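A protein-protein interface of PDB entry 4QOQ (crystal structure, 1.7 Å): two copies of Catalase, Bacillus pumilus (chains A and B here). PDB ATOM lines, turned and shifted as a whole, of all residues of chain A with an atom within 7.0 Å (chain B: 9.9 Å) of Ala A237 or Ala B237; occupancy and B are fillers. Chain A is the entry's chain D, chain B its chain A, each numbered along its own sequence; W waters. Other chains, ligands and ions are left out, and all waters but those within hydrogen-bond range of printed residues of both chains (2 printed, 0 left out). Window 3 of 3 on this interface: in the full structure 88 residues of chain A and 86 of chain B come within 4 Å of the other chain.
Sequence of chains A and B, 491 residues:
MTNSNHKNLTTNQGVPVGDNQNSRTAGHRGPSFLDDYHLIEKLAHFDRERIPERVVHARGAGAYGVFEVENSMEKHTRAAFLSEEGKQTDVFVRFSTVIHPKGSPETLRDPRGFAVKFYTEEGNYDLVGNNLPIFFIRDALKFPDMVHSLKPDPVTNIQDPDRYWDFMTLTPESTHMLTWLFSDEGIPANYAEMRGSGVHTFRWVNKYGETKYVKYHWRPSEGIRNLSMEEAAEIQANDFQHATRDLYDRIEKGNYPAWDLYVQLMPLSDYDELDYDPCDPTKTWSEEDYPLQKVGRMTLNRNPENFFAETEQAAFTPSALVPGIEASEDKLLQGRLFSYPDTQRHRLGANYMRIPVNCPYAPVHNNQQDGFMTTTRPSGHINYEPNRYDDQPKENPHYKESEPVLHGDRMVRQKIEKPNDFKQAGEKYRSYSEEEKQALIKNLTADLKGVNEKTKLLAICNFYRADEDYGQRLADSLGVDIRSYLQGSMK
NE2 of Gln B236 sits at hydrogen-bond distance from O of Gln A236.
The side-chain hydroxyl (OG1) of Thr A107 is in hydrogen-bond range of the side-chain amide oxygen (OE1) of Gln A236 (2.7 Å).
The side-chain amide oxygen of Gln B236 sits at hydrogen-bond distance from the side-chain hydroxyl of Thr B107.
Among the printed residues, pairs that only touch across the chains: Ala A233 with Ala B237 (3.4 Å), Ala A237 with Ala B233 (3.4 Å), Ala A237 with Gln B236 (3.5 Å), Gln A236 with Ala B237 (3.5 Å), Phe A240 with Pro B105 (3.7 Å), Ala A237 with Ala B237 (3.8 Å) and Phe A240 with Leu B108 (3.8 Å).
Of chain B, only Ala B233, Gln B236 and Ala B237 come within 4 Å of Ala A237.
Ala B237 touches just these residues of chain A: Ala A233, Gln A236 and Ala A237.
Ala A233 touches just one residue of chain B: Ala B237 (3.4 Å).
Gln A236 touches two residues of chain B.
No residue of chain B comes within 4 Å of Asn A238.
Printed residues of chain B within 4 Å of Phe A240: Pro B105 and Leu B108.
Of the printed residues of chain A, Gln B236 touches Gln A236 and Ala A237.
Printed residues of chain A within 4 Å of Pro B105: Phe A240 (3.7 Å).
Printed residues of chain A within 4 Å of Leu B108: Phe A240.
Printed residues of chain A within 4 Å of Ala B233: Ala A237 (3.4 Å).
The nearest residue of chain B that does not touch Ala A237 is Glu B234 (5.2 Å).
The nearest printed residue of chain B that does not touch Phe A240 is Gln B236 (4.3 Å).
Of the 12 printed residues of chain A, 4 touch a printed residue of chain B.
Hydrophobic or aromatic side chains of chain A within 4 Å of the printed part of chain B: Ala A233, Ala A237 and Phe A240.
Of the 20 printed residues of chain B, 5 touch a printed residue of chain A.
Hydrophobic or aromatic side chains of chain B within 4 Å of the printed part of chain A: Pro B105, Leu B108, Ala B233 and Ala B237.
Among the printed residues, 8 pairs touch across the chains.
Ala A233 touches Ala B237, and with the chains exchanged Ala A237 touches Ala B233.
Gln A236 touches its own counterpart, Gln B236.
Gln A236 touches Ala B237, and with the chains exchanged Ala A237 touches Gln B236.
Ala B237 touches its own counterpart, Ala A237.
Of the 8 pairs that touch across the chains among the printed residues, 6 have their exchanged pair printed and touching as well.
Water W1 lies within hydrogen-bond range of the side-chain amide nitrogen (NE2) of Gln A236 (3.0 Å) and the backbone carbonyl oxygen (O) of Asn B238 (3.2 Å).
Water W2 bridges NE2 of Gln B236 (3.1 Å) and O of Asn A238 (3.2 Å).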
ATOM      1  N   THR A 107      -0.465  20.958  23.781  1.00  0.00           N
ATOM      2  CA  THR A 107      -0.013  19.574  23.766  1.00  0.00           C
ATOM      3  C   THR A 107       0.294  18.987  22.356  1.00  0.00           C
ATOM      4  O   THR A 107       0.474  17.781  22.209  1.00  0.00           O
ATOM      5  CB  THR A 107      -1.077  18.734  24.493  1.00  0.00           C
ATOM      6  OG1 THR A 107      -2.371  19.157  24.036  1.00  0.00           O
ATOM      7  CG2 THR A 107      -0.988  18.971  25.967  1.00  0.00           C
ATOM      8  N   MET A 229       3.779  10.897  22.959  1.00  0.00           N
ATOM      9  CA  MET A 229       2.419  11.098  22.531  1.00  0.00           C
ATOM     10  C   MET A 229       1.429  10.807  23.614  1.00  0.00           C
ATOM     11  O   MET A 229       0.399  11.482  23.733  1.00  0.00           O
ATOM     12  CB  MET A 229       2.103  10.240  21.308  1.00  0.00           C
ATOM     13  CG  MET A 229       2.833  10.684  20.058  1.00  0.00           C
ATOM     14  SD  MET A 229       2.449   9.596  18.637  1.00  0.00           S
ATOM     15  CE  MET A 229       2.939   7.998  19.107  1.00  0.00           C
ATOM     16  N   GLU A 231       1.877  10.910  26.921  1.00  0.00           N
ATOM     17  CA  GLU A 231       1.931  11.904  27.980  1.00  0.00           C
ATOM     18  C   GLU A 231       1.175  13.183  27.500  1.00  0.00           C
ATOM     19  O   GLU A 231       0.461  13.817  28.322  1.00  0.00           O
ATOM     20  CB  GLU A 231       3.339  12.294  28.363  1.00  0.00           C
ATOM     21  CG  GLU A 231       4.118  11.255  29.188  1.00  0.00           C
ATOM     22  CD  GLU A 231       5.572  11.601  29.332  1.00  0.00           C
ATOM     23  OE1 GLU A 231       6.277  11.813  28.317  1.00  0.00           O
ATOM     24  OE2 GLU A 231       6.072  11.605  30.471  1.00  0.00           O
ATOM     25  N   ALA A 232       1.376  13.543  26.239  1.00  0.00           N
ATOM     26  CA  ALA A 232       0.706  14.729  25.677  1.00  0.00           C
ATOM     27  C   ALA A 232      -0.841  14.558  25.705  1.00  0.00           C
ATOM     28  O   ALA A 232      -1.557  15.467  26.110  1.00  0.00           O
ATOM     29  CB  ALA A 232       1.208  15.028  24.279  1.00  0.00           C
ATOM     30  N   ALA A 233      -1.334  13.395  25.310  1.00  0.00           N
ATOM     31  CA  ALA A 233      -2.760  13.131  25.335  1.00  0.00           C
ATOM     32  C   ALA A 233      -3.309  13.223  26.760  1.00  0.00           C
ATOM     33  O   ALA A 233      -4.374  13.736  26.956  1.00  0.00           O
ATOM     34  CB  ALA A 233      -3.057  11.751  24.728  1.00  0.00           C
ATOM     35  N   GLU A 234      -2.608  12.638  27.743  1.00  0.00           N
ATOM     36  CA  GLU A 234      -3.054  12.678  29.152  1.00  0.00           C
ATOM     37  C   GLU A 234      -3.155  14.113  29.692  1.00  0.00           C
ATOM     38  O   GLU A 234      -4.114  14.455  30.374  1.00  0.00           O
ATOM     39  CB  GLU A 234      -2.167  11.804  30.046  1.00  0.00           C
ATOM     40  CG  GLU A 234      -2.503  11.695  31.520  1.00  0.00           C
ATOM     41  CD  GLU A 234      -2.310  12.950  32.364  1.00  0.00           C
ATOM     42  OE1 GLU A 234      -3.150  13.252  33.322  1.00  0.00           O
ATOM     43  OE2 GLU A 234      -1.329  13.665  32.049  1.00  0.00           O
ATOM     44  N   ILE A 235      -2.231  14.979  29.296  1.00  0.00           N
ATOM     45  CA  ILE A 235      -2.329  16.410  29.668  1.00  0.00           C
ATOM     46  C   ILE A 235      -3.434  17.068  28.868  1.00  0.00           C
ATOM     47  O   ILE A 235      -4.297  17.782  29.473  1.00  0.00           O
ATOM     48  CB  ILE A 235      -0.974  17.156  29.415  1.00  0.00           C
ATOM     49  CG1 ILE A 235       0.083  16.653  30.402  1.00  0.00           C
ATOM     50  CG2 ILE A 235      -1.155  18.669  29.605  1.00  0.00           C
ATOM     51  CD1 ILE A 235       1.476  17.088  30.154  1.00  0.00           C
ATOM     52  N   GLN A 236      -3.520  16.762  27.569  1.00  0.00           N
ATOM     53  CA  GLN A 236      -4.581  17.390  26.746  1.00  0.00           C
ATOM     54  C   GLN A 236      -5.986  17.109  27.341  1.00  0.00           C
ATOM     55  O   GLN A 236      -6.925  17.947  27.247  1.00  0.00           O
ATOM     56  CB  GLN A 236      -4.499  16.929  25.320  1.00  0.00           C
ATOM     57  CG  GLN A 236      -5.336  17.737  24.353  1.00  0.00           C
ATOM     58  CD  GLN A 236      -5.037  17.403  22.925  1.00  0.00           C
ATOM     59  OE1 GLN A 236      -3.878  17.588  22.478  1.00  0.00           O
ATOM     60  NE2 GLN A 236      -5.994  16.848  22.200  1.00  0.00           N
ATOM     61  N   ALA A 237      -6.139  15.939  27.947  1.00  0.00           N
ATOM     62  CA  ALA A 237      -7.474  15.545  28.464  1.00  0.00           C
ATOM     63  C   ALA A 237      -8.023  16.532  29.489  1.00  0.00           C
ATOM     64  O   ALA A 237      -9.227  16.683  29.630  1.00  0.00           O
ATOM     65  CB  ALA A 237      -7.406  14.135  29.093  1.00  0.00           C
ATOM     66  N   ASN A 238      -7.136  17.107  30.278  1.00  0.00           N
ATOM     67  CA  ASN A 238      -7.528  17.937  31.414  1.00  0.00           C
ATOM     68  C   ASN A 238      -7.097  19.384  31.309  1.00  0.00           C
ATOM     69  O   ASN A 238      -7.604  20.210  32.036  1.00  0.00           O
ATOM     70  CB  ASN A 238      -6.916  17.398  32.701  1.00  0.00           C
ATOM     71  CG  ASN A 238      -7.393  16.006  33.029  1.00  0.00           C
ATOM     72  OD1 ASN A 238      -8.592  15.736  33.041  1.00  0.00           O
ATOM     73  ND2 ASN A 238      -6.465  15.110  33.266  1.00  0.00           N
ATOM     74  N   ASP A 239      -6.143  19.701  30.437  1.00  0.00           N
ATOM     75  CA  ASP A 239      -5.781  21.107  30.283  1.00  0.00           C
ATOM     76  C   ASP A 239      -5.326  21.405  28.869  1.00  0.00           C
ATOM     77  O   ASP A 239      -4.346  20.873  28.403  1.00  0.00           O
ATOM     78  CB  ASP A 239      -4.712  21.436  31.277  1.00  0.00           C
ATOM     79  CG  ASP A 239      -4.554  22.942  31.518  1.00  0.00           C
ATOM     80  OD1 ASP A 239      -5.201  23.778  30.815  1.00  0.00           O
ATOM     81  OD2 ASP A 239      -3.664  23.251  32.334  1.00  0.00           O
ATOM     82  N   PHE A 240      -5.990  22.306  28.191  1.00  0.00           N
ATOM     83  CA  PHE A 240      -5.542  22.663  26.832  1.00  0.00           C
ATOM     84  C   PHE A 240      -4.644  23.908  26.816  1.00  0.00           C
ATOM     85  O   PHE A 240      -4.377  24.482  25.741  1.00  0.00           O
ATOM     86  CB  PHE A 240      -6.749  22.814  25.846  1.00  0.00           C
ATOM     87  CG  PHE A 240      -7.687  23.890  26.188  1.00  0.00           C
ATOM     88  CD1 PHE A 240      -8.681  23.673  27.129  1.00  0.00           C
ATOM     89  CD2 PHE A 240      -7.661  25.094  25.539  1.00  0.00           C
ATOM     90  CE1 PHE A 240      -9.573  24.633  27.485  1.00  0.00           C
ATOM     91  CE2 PHE A 240      -8.555  26.076  25.923  1.00  0.00           C
ATOM     92  CZ  PHE A 240      -9.534  25.843  26.870  1.00  0.00           C
ATOM     93  N   PRO B 105     -11.103  23.375  22.132  1.00  0.00           N
ATOM     94  CA  PRO B 105     -11.770  22.096  22.061  1.00  0.00           C
ATOM     95  C   PRO B 105     -13.302  22.160  22.083  1.00  0.00           C
ATOM     96  O   PRO B 105     -13.921  23.041  22.679  1.00  0.00           O
ATOM     97  CB  PRO B 105     -11.255  21.354  23.309  1.00  0.00           C
ATOM     98  CG  PRO B 105     -10.018  22.080  23.711  1.00  0.00           C
ATOM     99  CD  PRO B 105     -10.187  23.495  23.287  1.00  0.00           C
ATOM    100  N   GLU B 106     -13.896  21.163  21.454  1.00  0.00           N
ATOM    101  CA  GLU B 106     -15.325  21.044  21.389  1.00  0.00           C
ATOM    102  C   GLU B 106     -15.942  20.128  22.464  1.00  0.00           C
ATOM    103  O   GLU B 106     -17.145  19.839  22.455  1.00  0.00           O
ATOM    104  CB  GLU B 106     -15.706  20.594  19.977  1.00  0.00           C
ATOM    105  CG  GLU B 106     -15.558  21.739  18.941  1.00  0.00           C
ATOM    106  CD  GLU B 106     -15.776  21.296  17.500  1.00  0.00           C
ATOM    107  OE1 GLU B 106     -15.378  20.171  17.149  1.00  0.00           O
ATOM    108  OE2 GLU B 106     -16.309  22.132  16.699  1.00  0.00           O
ATOM    109  N   THR B 107     -15.108  19.832  23.449  1.00  0.00           N
ATOM    110  CA  THR B 107     -15.453  19.043  24.642  1.00  0.00           C
ATOM    111  C   THR B 107     -15.650  19.883  25.909  1.00  0.00           C
ATOM    112  O   THR B 107     -15.790  19.345  27.004  1.00  0.00           O
ATOM    113  CB  THR B 107     -14.266  18.061  24.862  1.00  0.00           C
ATOM    114  OG1 THR B 107     -13.074  18.808  24.699  1.00  0.00           O
ATOM    115  CG2 THR B 107     -14.286  16.902  23.863  1.00  0.00           C
ATOM    116  N   LEU B 108     -15.600  21.221  25.796  1.00  0.00           N
ATOM    117  CA  LEU B 108     -15.789  22.121  26.915  1.00  0.00           C
ATOM    118  C   LEU B 108     -17.252  22.323  27.254  1.00  0.00           C
ATOM    119  O   LEU B 108     -18.115  22.199  26.387  1.00  0.00           O
ATOM    120  CB  LEU B 108     -15.157  23.482  26.602  1.00  0.00           C
ATOM    121  CG  LEU B 108     -13.676  23.469  26.147  1.00  0.00           C
ATOM    122  CD1 LEU B 108     -13.116  24.892  26.069  1.00  0.00           C
ATOM    123  CD2 LEU B 108     -12.832  22.698  27.145  1.00  0.00           C
ATOM    124  N   ILE B 187     -22.484  19.702  27.943  1.00  0.00           N
ATOM    125  CA  ILE B 187     -21.496  19.140  26.986  1.00  0.00           C
ATOM    126  C   ILE B 187     -22.256  18.179  26.082  1.00  0.00           C
ATOM    127  O   ILE B 187     -22.231  16.940  26.271  1.00  0.00           O
ATOM    128  CB  ILE B 187     -20.319  18.427  27.643  1.00  0.00           C
ATOM    129  CG1 ILE B 187     -19.755  19.229  28.847  1.00  0.00           C
ATOM    130  CG2 ILE B 187     -19.244  18.169  26.557  1.00  0.00           C
ATOM    131  CD1 ILE B 187     -18.569  18.562  29.530  1.00  0.00           C
ATOM    132  N   SER B 228     -20.638  13.100  30.068  1.00  0.00           N
ATOM    133  CA  SER B 228     -20.169  13.391  31.422  1.00  0.00           C
ATOM    134  C   SER B 228     -18.841  14.143  31.362  1.00  0.00           C
ATOM    135  O   SER B 228     -18.168  14.115  30.343  1.00  0.00           O
ATOM    136  CB  SER B 228     -20.038  12.081  32.254  1.00  0.00           C
ATOM    137  OG  SER B 228     -18.986  11.344  31.702  1.00  0.00           O
ATOM    138  N   MET B 229     -18.408  14.744  32.483  1.00  0.00           N
ATOM    139  CA  MET B 229     -17.104  15.296  32.515  1.00  0.00           C
ATOM    140  C   MET B 229     -16.012  14.304  32.160  1.00  0.00           C
ATOM    141  O   MET B 229     -15.083  14.632  31.449  1.00  0.00           O
ATOM    142  CB  MET B 229     -16.821  15.891  33.865  1.00  0.00           C
ATOM    143  CG  MET B 229     -17.644  17.103  34.212  1.00  0.00           C
ATOM    144  SD  MET B 229     -17.247  17.744  35.853  1.00  0.00           S
ATOM    145  CE  MET B 229     -15.510  18.131  35.625  1.00  0.00           C
ATOM    146  N   GLU B 230     -16.125  13.066  32.635  1.00  0.00           N
ATOM    147  CA  GLU B 230     -15.157  12.015  32.303  1.00  0.00           C
ATOM    148  C   GLU B 230     -15.175  11.612  30.839  1.00  0.00           C
ATOM    149  O   GLU B 230     -14.116  11.434  30.238  1.00  0.00           O
ATOM    150  CB  GLU B 230     -15.420  10.757  33.151  1.00  0.00           C
ATOM    151  CG  GLU B 230     -15.142  11.019  34.624  1.00  0.00           C
ATOM    152  CD  GLU B 230     -16.198  11.899  35.334  1.00  0.00           C
ATOM    153  OE1 GLU B 230     -17.405  12.073  34.877  1.00  0.00           O
ATOM    154  OE2 GLU B 230     -15.791  12.460  36.391  1.00  0.00           O
ATOM    155  N   GLU B 231     -16.366  11.532  30.246  1.00  0.00           N
ATOM    156  CA  GLU B 231     -16.478  11.164  28.815  1.00  0.00           C
ATOM    157  C   GLU B 231     -15.905  12.289  27.941  1.00  0.00           C
ATOM    158  O   GLU B 231     -15.196  12.033  26.957  1.00  0.00           O
ATOM    159  CB  GLU B 231     -17.901  10.935  28.381  1.00  0.00           C
ATOM    160  CG  GLU B 231     -18.539   9.635  28.858  1.00  0.00           C
ATOM    161  CD  GLU B 231     -20.047   9.582  28.557  1.00  0.00           C
ATOM    162  OE1 GLU B 231     -20.793  10.519  28.923  1.00  0.00           O
ATOM    163  OE2 GLU B 231     -20.472   8.611  27.882  1.00  0.00           O
ATOM    164  N   ALA B 232     -16.156  13.518  28.360  1.00  0.00           N
ATOM    165  CA  ALA B 232     -15.570  14.694  27.632  1.00  0.00           C
ATOM    166  C   ALA B 232     -14.060  14.706  27.670  1.00  0.00           C
ATOM    167  O   ALA B 232     -13.403  14.956  26.667  1.00  0.00           O
ATOM    168  CB  ALA B 232     -16.144  15.997  28.204  1.00  0.00           C
ATOM    169  N   ALA B 233     -13.475  14.419  28.849  1.00  0.00           N
ATOM    170  CA  ALA B 233     -12.024  14.380  28.988  1.00  0.00           C
ATOM    171  C   ALA B 233     -11.433  13.265  28.150  1.00  0.00           C
ATOM    172  O   ALA B 233     -10.386  13.482  27.498  1.00  0.00           O
ATOM    173  CB  ALA B 233     -11.620  14.223  30.442  1.00  0.00           C
ATOM    174  N   GLU B 234     -12.047  12.094  28.131  1.00  0.00           N
ATOM    175  CA  GLU B 234     -11.572  11.003  27.243  1.00  0.00           C
ATOM    176  C   GLU B 234     -11.484  11.384  25.745  1.00  0.00           C
ATOM    177  O   GLU B 234     -10.516  11.055  25.022  1.00  0.00           O
ATOM    178  CB  GLU B 234     -12.476   9.742  27.411  1.00  0.00           C
ATOM    179  CG  GLU B 234     -12.277   9.063  28.756  1.00  0.00           C
ATOM    180  CD  GLU B 234     -13.152   7.806  28.948  1.00  0.00           C
ATOM    181  OE1 GLU B 234     -13.031   7.184  30.037  1.00  0.00           O
ATOM    182  OE2 GLU B 234     -13.979   7.469  28.056  1.00  0.00           O
ATOM    183  N   ILE B 235     -12.526  12.070  25.272  1.00  0.00           N
ATOM    184  CA  ILE B 235     -12.560  12.568  23.877  1.00  0.00           C
ATOM    185  C   ILE B 235     -11.476  13.646  23.734  1.00  0.00           C
ATOM    186  O   ILE B 235     -10.721  13.639  22.766  1.00  0.00           O
ATOM    187  CB  ILE B 235     -13.968  13.091  23.474  1.00  0.00           C
ATOM    188  CG1 ILE B 235     -14.924  11.893  23.402  1.00  0.00           C
ATOM    189  CG2 ILE B 235     -13.904  13.765  22.100  1.00  0.00           C
ATOM    190  CD1 ILE B 235     -16.385  12.245  23.275  1.00  0.00           C
ATOM    191  N   GLN B 236     -11.409  14.563  24.683  1.00  0.00           N
ATOM    192  CA  GLN B 236     -10.494  15.706  24.543  1.00  0.00           C
ATOM    193  C   GLN B 236      -9.031  15.254  24.415  1.00  0.00           C
ATOM    194  O   GLN B 236      -8.228  15.883  23.696  1.00  0.00           O
ATOM    195  CB  GLN B 236     -10.634  16.665  25.733  1.00  0.00           C
ATOM    196  CG  GLN B 236      -9.935  17.987  25.539  1.00  0.00           C
ATOM    197  CD  GLN B 236     -10.279  18.972  26.616  1.00  0.00           C
ATOM    198  OE1 GLN B 236     -11.464  19.361  26.748  1.00  0.00           O
ATOM    199  NE2 GLN B 236      -9.307  19.391  27.410  1.00  0.00           N
ATOM    200  N   ALA B 237      -8.676  14.132  25.064  1.00  0.00           N
ATOM    201  CA  ALA B 237      -7.347  13.641  24.997  1.00  0.00           C
ATOM    202  C   ALA B 237      -6.871  13.398  23.582  1.00  0.00           C
ATOM    203  O   ALA B 237      -5.671  13.506  23.322  1.00  0.00           O
ATOM    204  CB  ALA B 237      -7.232  12.319  25.780  1.00  0.00           C
ATOM    205  N   ASN B 238      -7.784  12.931  22.719  1.00  0.00           N
ATOM    206  CA  ASN B 238      -7.400  12.494  21.380  1.00  0.00           C
ATOM    207  C   ASN B 238      -7.927  13.378  20.248  1.00  0.00           C
ATOM    208  O   ASN B 238      -7.422  13.286  19.154  1.00  0.00           O
ATOM    209  CB  ASN B 238      -7.867  11.071  21.141  1.00  0.00           C
ATOM    210  CG  ASN B 238      -7.203  10.077  22.095  1.00  0.00           C
ATOM    211  OD1 ASN B 238      -5.986  10.074  22.259  1.00  0.00           O
ATOM    212  ND2 ASN B 238      -8.001   9.299  22.756  1.00  0.00           N
ATOM    213  N   ASP B 239      -8.903  14.239  20.506  1.00  0.00           N
ATOM    214  CA  ASP B 239      -9.434  15.106  19.440  1.00  0.00           C
ATOM    215  C   ASP B 239      -9.993  16.382  20.034  1.00  0.00           C
ATOM    216  O   ASP B 239     -10.977  16.347  20.785  1.00  0.00           O
ATOM    217  CB  ASP B 239     -10.504  14.351  18.678  1.00  0.00           C
ATOM    218  CG  ASP B 239     -10.834  14.926  17.330  1.00  0.00           C
ATOM    219  OD1 ASP B 239     -10.319  16.032  16.978  1.00  0.00           O
ATOM    220  OD2 ASP B 239     -11.713  14.306  16.658  1.00  0.00           O
ATOM    221  N   PHE B 240      -9.444  17.498  19.631  1.00  0.00           N
ATOM    222  CA  PHE B 240      -9.992  18.811  20.065  1.00  0.00           C
ATOM    223  C   PHE B 240     -10.980  19.433  19.060  1.00  0.00           C
ATOM    224  O   PHE B 240     -11.407  20.523  19.243  1.00  0.00           O
ATOM    225  CB  PHE B 240      -8.834  19.752  20.432  1.00  0.00           C
ATOM    226  CG  PHE B 240      -7.978  20.128  19.316  1.00  0.00           C
ATOM    227  CD1 PHE B 240      -6.966  19.323  18.926  1.00  0.00           C
ATOM    228  CD2 PHE B 240      -8.175  21.306  18.639  1.00  0.00           C
ATOM    229  CE1 PHE B 240      -6.135  19.653  17.841  1.00  0.00           C
ATOM    230  CE2 PHE B 240      -7.343  21.661  17.550  1.00  0.00           C
ATOM    231  CZ  PHE B 240      -6.357  20.809  17.132  1.00  0.00           C
ATOM    232  N   GLN B 241     -11.351  18.715  18.012  1.00  0.00           N
ATOM    233  CA  GLN B 241     -12.324  19.171  17.041  1.00  0.00           C
ATOM    234  C   GLN B 241     -13.294  18.050  16.658  1.00  0.00           C
ATOM    235  O   GLN B 241     -13.719  17.900  15.520  1.00  0.00           O
ATOM    236  CB  GLN B 241     -11.657  19.817  15.816  1.00  0.00           C
ATOM    237  CG  GLN B 241     -10.885  18.859  14.955  1.00  0.00           C
ATOM    238  CD  GLN B 241      -9.375  19.045  15.075  1.00  0.00           C
ATOM    239  OE1 GLN B 241      -8.817  20.056  14.663  1.00  0.00           O
ATOM    240  NE2 GLN B 241      -8.719  18.060  15.633  1.00  0.00           N
ATOM    241  N   HIS B 242     -13.713  17.288  17.682  1.00  0.00           N
ATOM    242  CA  HIS B 242     -14.505  16.073  17.446  1.00  0.00           C
ATOM    243  C   HIS B 242     -15.886  16.363  16.851  1.00  0.00           C
ATOM    244  O   HIS B 242     -16.399  15.565  16.055  1.00  0.00           O
ATOM    245  CB  HIS B 242     -14.582  15.204  18.721  1.00  0.00           C
ATOM    246  CG  HIS B 242     -15.715  15.611  19.633  1.00  0.00           C
ATOM    247  ND1 HIS B 242     -15.651  16.717  20.450  1.00  0.00           N
ATOM    248  CD2 HIS B 242     -16.956  15.126  19.749  1.00  0.00           C
ATOM    249  CE1 HIS B 242     -16.792  16.861  21.085  1.00  0.00           C
ATOM    250  NE2 HIS B 242     -17.613  15.911  20.667  1.00  0.00           N
HETATM  251  O   HOH W   1      -5.877  16.076  19.294  1.00  0.00           O
HETATM  252  O   HOH W   2      -9.504  21.437  29.719  1.00  0.00           O
